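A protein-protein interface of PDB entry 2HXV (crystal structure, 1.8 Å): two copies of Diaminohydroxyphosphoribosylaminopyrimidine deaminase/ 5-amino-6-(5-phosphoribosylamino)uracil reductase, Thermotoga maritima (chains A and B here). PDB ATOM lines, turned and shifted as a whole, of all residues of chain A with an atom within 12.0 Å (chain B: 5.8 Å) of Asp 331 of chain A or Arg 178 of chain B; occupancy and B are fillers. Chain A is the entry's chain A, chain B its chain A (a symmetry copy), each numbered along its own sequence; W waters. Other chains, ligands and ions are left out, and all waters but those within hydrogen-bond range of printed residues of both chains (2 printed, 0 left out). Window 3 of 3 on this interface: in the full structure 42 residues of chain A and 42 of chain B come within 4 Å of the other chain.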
ATOM      1  N   LEU A 303      -6.884 -27.569  38.595  1.00  0.00           N
ATOM      2  CA  LEU A 303      -7.538 -28.118  37.425  1.00  0.00           C
ATOM      3  C   LEU A 303      -6.769 -29.310  36.880  1.00  0.00           C
ATOM      4  O   LEU A 303      -7.350 -30.347  36.583  1.00  0.00           O
ATOM      5  CB  LEU A 303      -7.647 -27.029  36.347  1.00  0.00           C
ATOM      6  CG  LEU A 303      -8.206 -27.552  35.024  1.00  0.00           C
ATOM      7  CD1 LEU A 303      -9.647 -27.853  35.191  1.00  0.00           C
ATOM      8  CD2 LEU A 303      -7.920 -26.530  33.961  1.00  0.00           C
ATOM      9  N   ASP A 304      -5.462 -29.186  36.751  1.00  0.00           N
ATOM     10  CA  ASP A 304      -4.620 -30.312  36.292  1.00  0.00           C
ATOM     11  C   ASP A 304      -4.512 -31.526  37.230  1.00  0.00           C
ATOM     12  O   ASP A 304      -3.904 -32.521  36.867  1.00  0.00           O
ATOM     13  CB  ASP A 304      -3.222 -29.834  35.910  1.00  0.00           C
ATOM     14  CG  ASP A 304      -3.222 -28.895  34.700  1.00  0.00           C
ATOM     15  OD1 ASP A 304      -4.112 -28.976  33.823  1.00  0.00           O
ATOM     16  OD2 ASP A 304      -2.298 -28.063  34.621  1.00  0.00           O
ATOM     17  N   PHE A 325     -11.415 -19.843  35.329  1.00  0.00           N
ATOM     18  CA  PHE A 325     -10.040 -20.309  35.408  1.00  0.00           C
ATOM     19  C   PHE A 325      -9.125 -19.191  35.026  1.00  0.00           C
ATOM     20  O   PHE A 325      -8.330 -19.311  34.109  1.00  0.00           O
ATOM     21  CB  PHE A 325      -9.840 -21.486  34.437  1.00  0.00           C
ATOM     22  CG  PHE A 325     -10.596 -22.709  34.801  1.00  0.00           C
ATOM     23  CD1 PHE A 325     -10.189 -23.449  35.900  1.00  0.00           C
ATOM     24  CD2 PHE A 325     -11.682 -23.171  34.041  1.00  0.00           C
ATOM     25  CE1 PHE A 325     -10.877 -24.586  36.262  1.00  0.00           C
ATOM     26  CE2 PHE A 325     -12.394 -24.304  34.410  1.00  0.00           C
ATOM     27  CZ  PHE A 325     -11.989 -25.028  35.530  1.00  0.00           C
ATOM     28  N   SER A 326      -9.257 -18.083  35.712  1.00  0.00           N
ATOM     29  CA  SER A 326      -8.640 -16.835  35.272  1.00  0.00           C
ATOM     30  C   SER A 326      -7.112 -16.929  35.388  1.00  0.00           C
ATOM     31  O   SER A 326      -6.395 -16.202  34.695  1.00  0.00           O
ATOM     32  CB  SER A 326      -9.143 -15.683  36.129  1.00  0.00           C
ATOM     33  OG  SER A 326      -8.666 -15.852  37.450  1.00  0.00           O
ATOM     34  N   GLY A 327      -6.628 -17.832  36.239  1.00  0.00           N
ATOM     35  CA  GLY A 327      -5.195 -18.074  36.383  1.00  0.00           C
ATOM     36  C   GLY A 327      -4.565 -19.052  35.403  1.00  0.00           C
ATOM     37  O   GLY A 327      -3.360 -19.212  35.386  1.00  0.00           O
ATOM     38  N   TYR A 328      -5.371 -19.729  34.600  1.00  0.00           N
ATOM     39  CA  TYR A 328      -4.902 -20.712  33.654  1.00  0.00           C
ATOM     40  C   TYR A 328      -4.607 -19.995  32.322  1.00  0.00           C
ATOM     41  O   TYR A 328      -5.045 -18.858  32.057  1.00  0.00           O
ATOM     42  CB  TYR A 328      -6.000 -21.743  33.448  1.00  0.00           C
ATOM     43  CG  TYR A 328      -5.610 -23.124  33.002  1.00  0.00           C
ATOM     44  CD1 TYR A 328      -5.142 -24.045  33.928  1.00  0.00           C
ATOM     45  CD2 TYR A 328      -5.847 -23.569  31.694  1.00  0.00           C
ATOM     46  CE1 TYR A 328      -4.814 -25.371  33.561  1.00  0.00           C
ATOM     47  CE2 TYR A 328      -5.514 -24.923  31.301  1.00  0.00           C
ATOM     48  CZ  TYR A 328      -5.008 -25.806  32.247  1.00  0.00           C
ATOM     49  OH  TYR A 328      -4.650 -27.128  31.958  1.00  0.00           O
ATOM     50  N   LEU A 329      -3.834 -20.643  31.485  1.00  0.00           N
ATOM     51  CA  LEU A 329      -3.676 -20.150  30.120  1.00  0.00           C
ATOM     52  C   LEU A 329      -3.417 -21.321  29.247  1.00  0.00           C
ATOM     53  O   LEU A 329      -2.553 -22.151  29.509  1.00  0.00           O
ATOM     54  CB  LEU A 329      -2.550 -19.122  29.949  1.00  0.00           C
ATOM     55  CG  LEU A 329      -2.555 -18.388  28.596  1.00  0.00           C
ATOM     56  CD1 LEU A 329      -3.816 -17.507  28.433  1.00  0.00           C
ATOM     57  CD2 LEU A 329      -1.300 -17.562  28.435  1.00  0.00           C
ATOM     58  N   SER A 330      -4.188 -21.382  28.193  1.00  0.00           N
ATOM     59  CA  SER A 330      -3.992 -22.362  27.184  1.00  0.00           C
ATOM     60  C   SER A 330      -4.323 -21.641  25.896  1.00  0.00           C
ATOM     61  O   SER A 330      -4.453 -20.412  25.882  1.00  0.00           O
ATOM     62  CB  SER A 330      -4.893 -23.566  27.444  1.00  0.00           C
ATOM     63  OG  SER A 330      -4.494 -24.614  26.598  1.00  0.00           O
ATOM     64  N   ASP A 331      -4.407 -22.394  24.820  1.00  0.00           N
ATOM     65  CA  ASP A 331      -4.759 -21.853  23.517  1.00  0.00           C
ATOM     66  C   ASP A 331      -5.391 -22.934  22.683  1.00  0.00           C
ATOM     67  O   ASP A 331      -5.406 -24.103  23.113  1.00  0.00           O
ATOM     68  CB  ASP A 331      -3.518 -21.241  22.837  1.00  0.00           C
ATOM     69  CG  ASP A 331      -2.471 -22.266  22.439  1.00  0.00           C
ATOM     70  OD1 ASP A 331      -2.797 -23.351  21.928  1.00  0.00           O
ATOM     71  OD2 ASP A 331      -1.280 -21.935  22.572  1.00  0.00           O
ATOM     72  N   VAL A 332      -5.888 -22.554  21.488  1.00  0.00           N
ATOM     73  CA  VAL A 332      -6.654 -23.463  20.620  1.00  0.00           C
ATOM     74  C   VAL A 332      -5.872 -24.691  20.253  1.00  0.00           C
ATOM     75  O   VAL A 332      -6.439 -25.678  19.910  1.00  0.00           O
ATOM     76  CB  VAL A 332      -7.105 -22.843  19.246  1.00  0.00           C
ATOM     77  CG1 VAL A 332      -8.032 -21.697  19.445  1.00  0.00           C
ATOM     78  CG2 VAL A 332      -5.894 -22.468  18.396  1.00  0.00           C
ATOM     79  N   SER A 333      -4.548 -24.646  20.285  1.00  0.00           N
ATOM     80  CA  SER A 333      -3.817 -25.807  19.817  1.00  0.00           C
ATOM     81  C   SER A 333      -3.726 -26.940  20.832  1.00  0.00           C
ATOM     82  O   SER A 333      -3.236 -28.020  20.500  1.00  0.00           O
ATOM     83  CB  SER A 333      -2.397 -25.398  19.427  1.00  0.00           C
ATOM     84  OG  SER A 333      -1.632 -25.277  20.611  1.00  0.00           O
ATOM     85  N   VAL A 334      -4.115 -26.698  22.076  1.00  0.00           N
ATOM     86  CA  VAL A 334      -3.999 -27.730  23.126  1.00  0.00           C
ATOM     87  C   VAL A 334      -5.259 -28.598  23.084  1.00  0.00           C
ATOM     88  O   VAL A 334      -6.357 -28.092  23.123  1.00  0.00           O
ATOM     89  CB  VAL A 334      -3.877 -27.138  24.506  1.00  0.00           C
ATOM     90  CG1 VAL A 334      -3.742 -28.261  25.554  1.00  0.00           C
ATOM     91  CG2 VAL A 334      -2.698 -26.171  24.559  1.00  0.00           C
ATOM     92  N   PRO A 335      -5.093 -29.907  22.953  1.00  0.00           N
ATOM     93  CA  PRO A 335      -6.295 -30.722  22.906  1.00  0.00           C
ATOM     94  C   PRO A 335      -7.017 -30.779  24.265  1.00  0.00           C
ATOM     95  O   PRO A 335      -6.426 -30.534  25.306  1.00  0.00           O
ATOM     96  CB  PRO A 335      -5.797 -32.108  22.497  1.00  0.00           C
ATOM     97  CG  PRO A 335      -4.301 -32.078  22.654  1.00  0.00           C
ATOM     98  CD  PRO A 335      -3.839 -30.664  22.813  1.00  0.00           C
ATOM     99  N   PRO A 336      -8.284 -31.147  24.239  1.00  0.00           N
ATOM    100  CA  PRO A 336      -9.061 -31.160  25.454  1.00  0.00           C
ATOM    101  C   PRO A 336      -8.559 -32.245  26.337  1.00  0.00           C
ATOM    102  O   PRO A 336      -8.149 -33.276  25.835  1.00  0.00           O
ATOM    103  CB  PRO A 336     -10.470 -31.491  24.982  1.00  0.00           C
ATOM    104  CG  PRO A 336     -10.402 -31.823  23.583  1.00  0.00           C
ATOM    105  CD  PRO A 336      -9.034 -31.587  23.061  1.00  0.00           C
ATOM    106  N   LYS A 337      -8.553 -31.986  27.617  1.00  0.00           N
ATOM    107  CA  LYS A 337      -8.054 -32.907  28.595  1.00  0.00           C
ATOM    108  C   LYS A 337      -9.155 -33.676  29.283  1.00  0.00           C
ATOM    109  O   LYS A 337      -8.850 -34.567  30.061  1.00  0.00           O
ATOM    110  CB  LYS A 337      -7.203 -32.171  29.601  1.00  0.00           C
ATOM    111  CG  LYS A 337      -5.979 -31.426  28.924  1.00  0.00           C
ATOM    112  CD  LYS A 337      -5.234 -32.283  27.894  1.00  0.00           C
ATOM    113  CE  LYS A 337      -4.089 -31.541  27.271  1.00  0.00           C
ATOM    114  NZ  LYS A 337      -3.723 -32.220  26.021  1.00  0.00           N
ATOM    115  N   ASP B 176      -9.112 -17.746  21.779  1.00  0.00           N
ATOM    116  CA  ASP B 176      -8.029 -17.716  22.782  1.00  0.00           C
ATOM    117  C   ASP B 176      -7.378 -16.336  22.851  1.00  0.00           C
ATOM    118  O   ASP B 176      -7.851 -15.343  22.292  1.00  0.00           O
ATOM    119  CB  ASP B 176      -7.037 -18.815  22.534  1.00  0.00           C
ATOM    120  CG  ASP B 176      -6.175 -18.575  21.285  1.00  0.00           C
ATOM    121  OD1 ASP B 176      -6.155 -17.431  20.714  1.00  0.00           O
ATOM    122  OD2 ASP B 176      -5.533 -19.559  20.894  1.00  0.00           O
ATOM    123  N   HIS B 177      -6.307 -16.250  23.620  1.00  0.00           N
ATOM    124  CA  HIS B 177      -5.668 -14.954  23.857  1.00  0.00           C
ATOM    125  C   HIS B 177      -5.098 -14.311  22.614  1.00  0.00           C
ATOM    126  O   HIS B 177      -4.857 -13.099  22.618  1.00  0.00           O
ATOM    127  CB  HIS B 177      -4.591 -15.103  24.916  1.00  0.00           C
ATOM    128  CG  HIS B 177      -3.425 -15.920  24.475  1.00  0.00           C
ATOM    129  ND1 HIS B 177      -2.244 -15.343  24.067  1.00  0.00           N
ATOM    130  CD2 HIS B 177      -3.237 -17.261  24.401  1.00  0.00           C
ATOM    131  CE1 HIS B 177      -1.390 -16.293  23.735  1.00  0.00           C
ATOM    132  NE2 HIS B 177      -1.963 -17.464  23.931  1.00  0.00           N
ATOM    133  N   ARG B 178      -4.877 -15.097  21.565  1.00  0.00           N
ATOM    134  CA  ARG B 178      -4.419 -14.585  20.269  1.00  0.00           C
ATOM    135  C   ARG B 178      -5.562 -14.266  19.285  1.00  0.00           C
ATOM    136  O   ARG B 178      -5.304 -13.845  18.143  1.00  0.00           O
ATOM    137  CB  ARG B 178      -3.518 -15.615  19.600  1.00  0.00           C
ATOM    138  CG  ARG B 178      -2.290 -15.932  20.374  1.00  0.00           C
ATOM    139  CD  ARG B 178      -1.231 -16.528  19.469  1.00  0.00           C
ATOM    140  NE  ARG B 178      -1.290 -17.983  19.438  1.00  0.00           N
ATOM    141  CZ  ARG B 178      -0.683 -18.788  20.317  1.00  0.00           C
ATOM    142  NH1 ARG B 178       0.049 -18.290  21.313  1.00  0.00           N
ATOM    143  NH2 ARG B 178      -0.806 -20.108  20.197  1.00  0.00           N
ATOM    144  N   GLY B 179      -6.813 -14.468  19.723  1.00  0.00           N
ATOM    145  CA  GLY B 179      -7.981 -14.289  18.889  1.00  0.00           C
ATOM    146  C   GLY B 179      -8.254 -15.481  17.994  1.00  0.00           C
ATOM    147  O   GLY B 179      -9.042 -15.357  17.086  1.00  0.00           O
ATOM    148  N   ASP B 180      -7.603 -16.620  18.253  1.00  0.00           N
ATOM    149  CA  ASP B 180      -7.725 -17.827  17.424  1.00  0.00           C
ATOM    150  C   ASP B 180      -8.992 -18.548  17.895  1.00  0.00           C
ATOM    151  O   ASP B 180      -9.171 -18.687  19.102  1.00  0.00           O
ATOM    152  CB  ASP B 180      -6.568 -18.799  17.665  1.00  0.00           C
ATOM    153  CG  ASP B 180      -5.394 -18.639  16.678  1.00  0.00           C
ATOM    154  OD1 ASP B 180      -5.555 -19.051  15.498  1.00  0.00           O
ATOM    155  OD2 ASP B 180      -4.299 -18.184  17.123  1.00  0.00           O
ATOM    156  N   LYS B 211     -11.100 -11.602  10.862  1.00  0.00           N
ATOM    157  CA  LYS B 211     -10.218 -12.451  11.666  1.00  0.00           C
ATOM    158  C   LYS B 211     -10.133 -13.872  11.139  1.00  0.00           C
ATOM    159  O   LYS B 211      -9.041 -14.422  10.976  1.00  0.00           O
ATOM    160  CB  LYS B 211     -10.639 -12.399  13.133  1.00  0.00           C
ATOM    161  CG  LYS B 211      -9.773 -13.343  14.046  1.00  0.00           C
ATOM    162  CD  LYS B 211      -8.284 -12.990  14.105  1.00  0.00           C
ATOM    163  CE  LYS B 211      -7.442 -14.167  14.650  1.00  0.00           C
ATOM    164  NZ  LYS B 211      -6.039 -13.717  14.927  1.00  0.00           N
ATOM    165  N   LYS B 316     -12.269 -27.853  26.341  1.00  0.00           N
ATOM    166  CA  LYS B 316     -11.142 -26.964  26.328  1.00  0.00           C
ATOM    167  C   LYS B 316     -11.362 -25.837  27.322  1.00  0.00           C
ATOM    168  O   LYS B 316     -12.489 -25.455  27.622  1.00  0.00           O
ATOM    169  CB  LYS B 316     -10.897 -26.386  24.939  1.00  0.00           C
ATOM    170  CG  LYS B 316     -10.326 -27.401  23.965  1.00  0.00           C
ATOM    171  CD  LYS B 316     -10.075 -26.839  22.584  1.00  0.00           C
ATOM    172  CE  LYS B 316      -9.490 -27.968  21.724  1.00  0.00           C
ATOM    173  NZ  LYS B 316      -9.534 -27.548  20.284  1.00  0.00           N
ATOM    174  N   ILE B 317     -10.255 -25.296  27.809  1.00  0.00           N
ATOM    175  CA  ILE B 317     -10.238 -24.212  28.753  1.00  0.00           C
ATOM    176  C   ILE B 317      -9.156 -23.287  28.263  1.00  0.00           C
ATOM    177  O   ILE B 317      -8.023 -23.734  28.138  1.00  0.00           O
ATOM    178  CB  ILE B 317      -9.860 -24.738  30.172  1.00  0.00           C
ATOM    179  CG1 ILE B 317     -10.955 -25.650  30.709  1.00  0.00           C
ATOM    180  CG2 ILE B 317      -9.609 -23.570  31.102  1.00  0.00           C
ATOM    181  CD1 ILE B 317     -10.591 -26.400  32.000  1.00  0.00           C
ATOM    182  N   PHE B 318      -9.463 -22.017  28.018  1.00  0.00           N
ATOM    183  CA  PHE B 318      -8.451 -21.083  27.487  1.00  0.00           C
ATOM    184  C   PHE B 318      -7.846 -20.185  28.570  1.00  0.00           C
ATOM    185  O   PHE B 318      -6.774 -19.625  28.382  1.00  0.00           O
ATOM    186  CB  PHE B 318      -8.987 -20.177  26.374  1.00  0.00           C
ATOM    187  CG  PHE B 318      -9.277 -20.886  25.056  1.00  0.00           C
ATOM    188  CD1 PHE B 318      -8.791 -22.149  24.777  1.00  0.00           C
ATOM    189  CD2 PHE B 318     -10.051 -20.249  24.103  1.00  0.00           C
ATOM    190  CE1 PHE B 318      -9.103 -22.767  23.555  1.00  0.00           C
ATOM    191  CE2 PHE B 318     -10.347 -20.838  22.915  1.00  0.00           C
ATOM    192  CZ  PHE B 318      -9.872 -22.117  22.641  1.00  0.00           C
HETATM  193  O   HOH W   1      -5.973 -18.178  25.592  1.00  0.00           O
HETATM  194  O   HOH W   2      -0.314 -20.197  25.136  1.00  0.00           O
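Ile 317 of chain B touches Leu 303 of chain A. Ile 317 of chain B touches Tyr 328 of chain A. Leu 329 of chain A touches Phe 318 of chain B (CA to O, 3.6 Å). His 177 of chain B touches Ser 330 of chain A (CD2 to O, 3.7 Å). Asp 176 of chain B touches Asp 331 of chain A. CE1 of Phe 318 of chain B touches C of Asp 331 of chain A, 3.8 Å away. Val 332 of chain A touches Lys 316 of chain B. CZ of Phe 318 of chain B touches CG1 of Val 332 of chain A, 3.7 Å away. CE of Lys 316 of chain B touches O of Val 334 of chain A, 3.4 Å away. Lys 316 of chain B touches Pro 336 of chain A.
Hydrophobic or aromatic side chains of chain B within 4 Å of the printed part of chain A: His 177, Ile 317 and Phe 318. Printed residues of chain A that touch a printed residue of chain B: Leu 303, Phe 325, Tyr 328, Leu 329, Ser 330, Asp 331, Val 332, Val 334 and Pro 336. Among the printed residues, 16 pairs touch across the chains. Among the printed residues, Asp or Glu carboxylates within 4 Å of a Lys or Arg side-chain nitrogen of the other chain: Asp 331 of chain A with Arg 178 of chain B (3.0 Å).
The backbone NH (N) of Ser 330 of chain A is in hydrogen-bond range of the backbone carbonyl oxygen (O) of Phe 318 of chain B (3.1 Å). The guanidinium group (NH2) of Arg 178 of chain B is in salt-bridge range of the side-chain carboxylate (OD2) of Asp 331 of chain A, at 3.0 Å. The backbone NH (N) of Val 332 of chain A sits at hydrogen-bond distance from the side-chain carboxylate (OD2) of Asp 176 of chain B, 3.1 Å away.
The backbone carbonyl oxygen (O) of Arg 178 of chain B lies within hydrogen-bond range of the side-chain amino group (NZ) of Lys 211 of chain B (3.3 Å). NH1 of Arg 178 of chain B lies within hydrogen-bond range of NE2 of His 177 of chain B (3.4 Å). OD2 of Asp 180 of chain B lies within salt-bridge range of NE of Arg 178 of chain B, 3.8 Å away. The side-chain carboxylate of Asp 176 of chain B is in hydrogen-bond range of the backbone NH of Arg 178 of chain B (2.8 Å). The side-chain carboxylate (OD1) of Asp 176 of chain B lies within hydrogen-bond range of the backbone NH (N) of Asp 180 of chain B (3.0 Å). OD1 of Asp 331 of chain A sits at hydrogen-bond distance from OG of Ser 333 of chain A (2.6 Å).
No position is printed for both chains. Of the 16 pairs that touch across the chains among the printed residues, none has its exchanged pair printed and touching as well.
Water W1 lies within hydrogen-bond range of the backbone carbonyl oxygen of Ser 330 of chain A (2.7 Å), the backbone NH of His 177 of chain B (2.8 Å) and the backbone carbonyl oxygen of Phe 318 of chain B (3.2 Å). Water W2 bridges OD2 of Asp 331 of chain A and NE2 of His 177 of chain B.
Printed residues of chain B within 4 Å of Leu 329 of chain A: Phe 318. Printed residues of chain B within 4 Å of Ser 330 of chain A: His 177 (3.7 Å), Ile 317 (3.2 Å) and Phe 318 (3.1 Å). Of chain B, only Asp 176, Arg 178 and Phe 318 come within 4 Å of Asp 331 of chain A. Ser 333 of chain A touches none of the printed residues of chain B. Printed residues of chain B within 4 Å of Pro 336 of chain A: Lys 316 (3.9 Å). Lys 337 of chain A touches none of the printed residues of chain B. Of chain A, only Asp 331 (3.3 Å) and Val 332 (3.1 Å) come within 4 Å of Asp 176 of chain B. Of chain A, only Ser 330 (3.7 Å) comes within 4 Å of His 177 of chain B. Of the printed residues of chain A, Arg 178 of chain B touches Asp 331. Of chain A, only Val 332 comes within 4 Å of Asp 180 of chain B. Printed residues of chain A within 4 Å of Lys 316 of chain B: Val 332, Val 334 and Pro 336. Printed residues of chain A within 4 Å of Ile 317 of chain B: Leu 303 (3.3 Å), Phe 325 (3.6 Å), Tyr 328 (3.8 Å) and Ser 330 (3.2 Å). Phe 318 of chain B touches just these residues of chain A: Leu 329 (3.6 Å), Ser 330 (3.1 Å), Asp 331 (3.8 Å) and Val 332 (3.7 Å). The nearest printed residue of chain B that does not touch Leu 303 of chain A is Lys 316 of chain B (7.5 Å).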
